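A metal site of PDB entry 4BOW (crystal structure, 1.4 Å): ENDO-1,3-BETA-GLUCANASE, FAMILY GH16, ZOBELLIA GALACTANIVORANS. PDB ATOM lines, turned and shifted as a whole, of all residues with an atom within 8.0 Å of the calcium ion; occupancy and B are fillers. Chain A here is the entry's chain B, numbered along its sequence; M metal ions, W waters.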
ATOM      1  N   ASP A  17     -24.937  23.972  17.507  1.00  0.00           N
ATOM      2  CA  ASP A  17     -24.963  25.058  16.535  1.00  0.00           C
ATOM      3  C   ASP A  17     -23.923  24.800  15.432  1.00  0.00           C
ATOM      4  O   ASP A  17     -22.719  24.695  15.761  1.00  0.00           O
ATOM      5  CB  ASP A  17     -24.823  26.380  17.248  1.00  0.00           C
ATOM      6  CG  ASP A  17     -25.279  27.571  16.395  1.00  0.00           C
ATOM      7  OD1 ASP A  17     -25.361  27.439  15.126  1.00  0.00           O
ATOM      8  OD2 ASP A  17     -25.461  28.630  17.011  1.00  0.00           O
ATOM      9  N   GLU A  18     -24.362  24.766  14.163  1.00  0.00           N
ATOM     10  CA  GLU A  18     -23.444  24.569  13.007  1.00  0.00           C
ATOM     11  C   GLU A  18     -22.974  25.861  12.458  1.00  0.00           C
ATOM     12  O   GLU A  18     -22.104  25.886  11.552  1.00  0.00           O
ATOM     13  CB  GLU A  18     -24.130  23.769  11.896  1.00  0.00           C
ATOM     14  CG  GLU A  18     -24.602  22.395  12.448  1.00  0.00           C
ATOM     15  CD  GLU A  18     -23.452  21.421  12.809  1.00  0.00           C
ATOM     16  OE1 GLU A  18     -22.361  21.473  12.190  1.00  0.00           O
ATOM     17  OE2 GLU A  18     -23.661  20.546  13.685  1.00  0.00           O
ATOM     18  N   PHE A  19     -23.575  26.927  12.998  1.00  0.00           N
ATOM     19  CA  PHE A  19     -23.179  28.321  12.676  1.00  0.00           C
ATOM     20  C   PHE A  19     -23.296  28.554  11.163  1.00  0.00           C
ATOM     21  O   PHE A  19     -22.453  29.251  10.581  1.00  0.00           O
ATOM     22  CB  PHE A  19     -21.766  28.627  13.240  1.00  0.00           C
ATOM     23  CG  PHE A  19     -21.741  28.653  14.755  1.00  0.00           C
ATOM     24  CD1 PHE A  19     -22.458  29.623  15.488  1.00  0.00           C
ATOM     25  CD2 PHE A  19     -20.968  27.732  15.470  1.00  0.00           C
ATOM     26  CE1 PHE A  19     -22.491  29.619  16.898  1.00  0.00           C
ATOM     27  CE2 PHE A  19     -20.979  27.752  16.935  1.00  0.00           C
ATOM     28  CZ  PHE A  19     -21.707  28.681  17.623  1.00  0.00           C
ATOM     29  N   GLU A  20     -24.304  27.929  10.542  1.00  0.00           N
ATOM     30  CA  GLU A  20     -24.497  28.034   9.078  1.00  0.00           C
ATOM     31  C   GLU A  20     -25.567  29.067   8.905  1.00  0.00           C
ATOM     32  O   GLU A  20     -26.545  28.815   8.190  1.00  0.00           O
ATOM     33  CB  GLU A  20     -24.839  26.670   8.443  1.00  0.00           C
ATOM     34  CG  GLU A  20     -23.790  25.523   8.544  1.00  0.00           C
ATOM     35  CD  GLU A  20     -22.451  25.755   7.832  1.00  0.00           C
ATOM     36  OE1 GLU A  20     -22.387  26.420   6.735  1.00  0.00           O
ATOM     37  OE2 GLU A  20     -21.422  25.232   8.392  1.00  0.00           O
ATOM     38  N   TYR A  21     -25.416  30.247   9.500  1.00  0.00           N
ATOM     39  CA  TYR A  21     -26.230  31.453   9.262  1.00  0.00           C
ATOM     40  C   TYR A  21     -25.319  32.680   9.253  1.00  0.00           C
ATOM     41  O   TYR A  21     -24.097  32.579   9.318  1.00  0.00           O
ATOM     42  CB  TYR A  21     -27.415  31.661  10.268  1.00  0.00           C
ATOM     43  CG  TYR A  21     -26.963  31.491  11.725  1.00  0.00           C
ATOM     44  CD1 TYR A  21     -27.005  30.260  12.271  1.00  0.00           C
ATOM     45  CD2 TYR A  21     -26.579  32.607  12.520  1.00  0.00           C
ATOM     46  CE1 TYR A  21     -26.486  30.091  13.630  1.00  0.00           C
ATOM     47  CE2 TYR A  21     -26.104  32.464  13.853  1.00  0.00           C
ATOM     48  CZ  TYR A  21     -26.110  31.220  14.438  1.00  0.00           C
ATOM     49  OH  TYR A  21     -25.578  31.068  15.788  1.00  0.00           O
ATOM     50  N   VAL A  59     -21.368  35.518  13.204  1.00  0.00           N
ATOM     51  CA  VAL A  59     -21.400  34.266  12.478  1.00  0.00           C
ATOM     52  C   VAL A  59     -21.429  34.569  11.001  1.00  0.00           C
ATOM     53  O   VAL A  59     -22.214  35.430  10.549  1.00  0.00           O
ATOM     54  CB  VAL A  59     -22.657  33.394  12.934  1.00  0.00           C
ATOM     55  CG1 VAL A  59     -22.585  31.995  12.321  1.00  0.00           C
ATOM     56  CG2 VAL A  59     -22.657  33.270  14.460  1.00  0.00           C
ATOM     57  N   SER A  60     -20.578  33.887  10.222  1.00  0.00           N
ATOM     58  CA  SER A  60     -20.543  34.157   8.794  1.00  0.00           C
ATOM     59  C   SER A  60     -19.718  33.067   8.149  1.00  0.00           C
ATOM     60  O   SER A  60     -18.805  32.490   8.813  1.00  0.00           O
ATOM     61  CB  SER A  60     -20.022  35.574   8.538  1.00  0.00           C
ATOM     62  OG  SER A  60     -18.832  35.859   9.254  1.00  0.00           O
ATOM     63  N   ASP A  61     -20.080  32.693   6.902  1.00  0.00           N
ATOM     64  CA  ASP A  61     -19.260  31.750   6.133  1.00  0.00           C
ATOM     65  C   ASP A  61     -19.114  30.374   6.801  1.00  0.00           C
ATOM     66  O   ASP A  61     -18.136  29.633   6.574  1.00  0.00           O
ATOM     67  CB  ASP A  61     -17.957  32.431   5.778  1.00  0.00           C
ATOM     68  CG  ASP A  61     -18.214  33.641   4.949  1.00  0.00           C
ATOM     69  OD1 ASP A  61     -18.763  33.415   3.850  1.00  0.00           O
ATOM     70  OD2 ASP A  61     -17.998  34.787   5.401  1.00  0.00           O
ATOM     71  N   GLY A  62     -20.153  30.024   7.542  1.00  0.00           N
ATOM     72  CA  GLY A  62     -20.230  28.737   8.265  1.00  0.00           C
ATOM     73  C   GLY A  62     -19.515  28.588   9.613  1.00  0.00           C
ATOM     74  O   GLY A  62     -19.424  27.462  10.143  1.00  0.00           O
ATOM     75  N   THR A  63     -19.030  29.684  10.178  1.00  0.00           N
ATOM     76  CA  THR A  63     -18.308  29.640  11.470  1.00  0.00           C
ATOM     77  C   THR A  63     -18.675  30.825  12.386  1.00  0.00           C
ATOM     78  O   THR A  63     -18.973  31.967  11.920  1.00  0.00           O
ATOM     79  CB  THR A  63     -16.783  29.593  11.259  1.00  0.00           C
ATOM     80  OG1 THR A  63     -16.353  30.837  10.700  1.00  0.00           O
ATOM     81  CG2 THR A  63     -16.332  28.422  10.450  1.00  0.00           C
ATOM     82  N   LEU A  64     -18.665  30.585  13.719  1.00  0.00           N
ATOM     83  CA  LEU A  64     -18.761  31.662  14.699  1.00  0.00           C
ATOM     84  C   LEU A  64     -17.334  32.243  14.937  1.00  0.00           C
ATOM     85  O   LEU A  64     -16.332  31.487  14.919  1.00  0.00           O
ATOM     86  CB  LEU A  64     -19.219  31.120  16.113  1.00  0.00           C
ATOM     87  CG  LEU A  64     -18.983  31.988  17.382  1.00  0.00           C
ATOM     88  CD1 LEU A  64     -19.848  33.321  17.441  1.00  0.00           C
ATOM     89  CD2 LEU A  64     -19.205  31.111  18.636  1.00  0.00           C
ATOM     90  N   ARG A 101     -15.423  22.163  17.170  1.00  0.00           N
ATOM     91  CA  ARG A 101     -14.432  22.262  16.094  1.00  0.00           C
ATOM     92  C   ARG A 101     -14.053  23.710  15.929  1.00  0.00           C
ATOM     93  O   ARG A 101     -14.929  24.543  15.699  1.00  0.00           O
ATOM     94  CB  ARG A 101     -14.943  21.632  14.817  1.00  0.00           C
ATOM     95  CG  ARG A 101     -13.884  21.651  13.695  1.00  0.00           C
ATOM     96  CD  ARG A 101     -14.371  20.746  12.545  1.00  0.00           C
ATOM     97  NE  ARG A 101     -13.284  20.505  11.569  1.00  0.00           N
ATOM     98  CZ  ARG A 101     -13.215  21.033  10.346  1.00  0.00           C
ATOM     99  NH1 ARG A 101     -14.132  21.908   9.946  1.00  0.00           N
ATOM    100  NH2 ARG A 101     -12.188  20.719   9.549  1.00  0.00           N
ATOM    101  N   PHE A 186      -8.402  23.663  11.716  1.00  0.00           N
ATOM    102  CA  PHE A 186      -9.433  23.303  12.666  1.00  0.00           C
ATOM    103  C   PHE A 186      -8.955  22.008  13.418  1.00  0.00           C
ATOM    104  O   PHE A 186      -8.320  21.111  12.823  1.00  0.00           O
ATOM    105  CB  PHE A 186     -10.803  23.027  11.958  1.00  0.00           C
ATOM    106  CG  PHE A 186     -11.553  24.299  11.535  1.00  0.00           C
ATOM    107  CD1 PHE A 186     -12.275  25.074  12.485  1.00  0.00           C
ATOM    108  CD2 PHE A 186     -11.599  24.684  10.156  1.00  0.00           C
ATOM    109  CE1 PHE A 186     -12.948  26.215  12.173  1.00  0.00           C
ATOM    110  CE2 PHE A 186     -12.316  25.835   9.834  1.00  0.00           C
ATOM    111  CZ  PHE A 186     -12.982  26.586  10.816  1.00  0.00           C
ATOM    112  N   ILE A 249     -15.030  29.187  15.451  1.00  0.00           N
ATOM    113  CA  ILE A 249     -15.643  27.926  15.850  1.00  0.00           C
ATOM    114  C   ILE A 249     -16.610  27.438  14.715  1.00  0.00           C
ATOM    115  O   ILE A 249     -17.566  28.135  14.392  1.00  0.00           O
ATOM    116  CB  ILE A 249     -16.397  28.099  17.163  1.00  0.00           C
ATOM    117  CG1 ILE A 249     -15.368  28.400  18.280  1.00  0.00           C
ATOM    118  CG2 ILE A 249     -17.172  26.800  17.520  1.00  0.00           C
ATOM    119  CD1 ILE A 249     -15.940  28.927  19.512  1.00  0.00           C
ATOM    120  N   ASP A 250     -16.312  26.275  14.143  1.00  0.00           N
ATOM    121  CA  ASP A 250     -17.085  25.643  13.038  1.00  0.00           C
ATOM    122  C   ASP A 250     -18.454  25.135  13.583  1.00  0.00           C
ATOM    123  O   ASP A 250     -19.509  25.313  12.928  1.00  0.00           O
ATOM    124  CB  ASP A 250     -16.309  24.486  12.428  1.00  0.00           C
ATOM    125  CG  ASP A 250     -16.941  23.939  11.188  1.00  0.00           C
ATOM    126  OD1 ASP A 250     -17.820  24.625  10.562  1.00  0.00           O
ATOM    127  OD2 ASP A 250     -16.571  22.781  10.838  1.00  0.00           O
ATOM    128  N   TYR A 251     -18.468  24.512  14.783  1.00  0.00           N
ATOM    129  CA  TYR A 251     -19.719  23.995  15.340  1.00  0.00           C
ATOM    130  C   TYR A 251     -19.497  23.649  16.820  1.00  0.00           C
ATOM    131  O   TYR A 251     -18.344  23.457  17.300  1.00  0.00           O
ATOM    132  CB  TYR A 251     -20.225  22.744  14.601  1.00  0.00           C
ATOM    133  CG  TYR A 251     -19.282  21.576  14.553  1.00  0.00           C
ATOM    134  CD1 TYR A 251     -19.034  20.799  15.729  1.00  0.00           C
ATOM    135  CD2 TYR A 251     -18.676  21.176  13.356  1.00  0.00           C
ATOM    136  CE1 TYR A 251     -18.179  19.700  15.691  1.00  0.00           C
ATOM    137  CE2 TYR A 251     -17.849  20.096  13.280  1.00  0.00           C
ATOM    138  CZ  TYR A 251     -17.613  19.331  14.418  1.00  0.00           C
ATOM    139  OH  TYR A 251     -16.753  18.287  14.296  1.00  0.00           O
ATOM    140  N   VAL A 252     -20.586  23.601  17.516  1.00  0.00           N
ATOM    141  CA  VAL A 252     -20.690  22.996  18.876  1.00  0.00           C
ATOM    142  C   VAL A 252     -21.714  21.858  18.730  1.00  0.00           C
ATOM    143  O   VAL A 252     -22.808  22.062  18.149  1.00  0.00           O
ATOM    144  CB  VAL A 252     -21.158  24.022  19.887  1.00  0.00           C
ATOM    145  CG1 VAL A 252     -21.462  23.384  21.253  1.00  0.00           C
ATOM    146  CG2 VAL A 252     -20.155  25.173  20.053  1.00  0.00           C
ATOM    147  N   ARG A 253     -21.403  20.645  19.183  1.00  0.00           N
ATOM    148  CA  ARG A 253     -22.378  19.535  19.156  1.00  0.00           C
ATOM    149  C   ARG A 253     -22.298  18.903  20.559  1.00  0.00           C
ATOM    150  O   ARG A 253     -21.200  18.618  21.050  1.00  0.00           O
ATOM    151  CB  ARG A 253     -21.981  18.514  18.057  1.00  0.00           C
ATOM    152  CG  ARG A 253     -22.213  19.047  16.633  1.00  0.00           C
ATOM    153  CD  ARG A 253     -21.649  18.095  15.643  1.00  0.00           C
ATOM    154  NE  ARG A 253     -21.680  18.681  14.290  1.00  0.00           N
ATOM    155  CZ  ARG A 253     -20.943  18.219  13.282  1.00  0.00           C
ATOM    156  NH1 ARG A 253     -20.185  17.115  13.406  1.00  0.00           N
ATOM    157  NH2 ARG A 253     -21.000  18.875  12.125  1.00  0.00           N
HETATM  158 CA    CA M   1     -20.087  25.385  10.682  1.00  0.00          CA
HETATM  159  O   HOH W   1     -20.781  23.021  10.727  1.00  0.00           O
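NE of Arg 253 is in salt-bridge range of OE2 of Glu 18, at 2.8 Å. The guanidinium group of Arg 101 lies within salt-bridge range of the side-chain carboxylate of Asp 250, 2.7 Å away.
Within 4 Å of the calcium ion: Glu 18, Glu 20, Gly 62 and Asp 250.
The backbone carbonyl oxygen (O) of Gly 62 binds the calcium ion. O of Glu 18 binds the calcium ion (2.3 Å). The calcium ion is bound by the backbone carbonyl oxygen (O) of Asp 250 (2.3 Å). The side-chain carboxylate (OD1) of Asp 250 binds the calcium ion (2.4 Å). Water W1 is bound to the calcium ion, 2.5 Å away. The calcium ion is bound by OE2 of Glu 20 (2.7 Å). The calcium ion has six donor atoms within binding distance.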
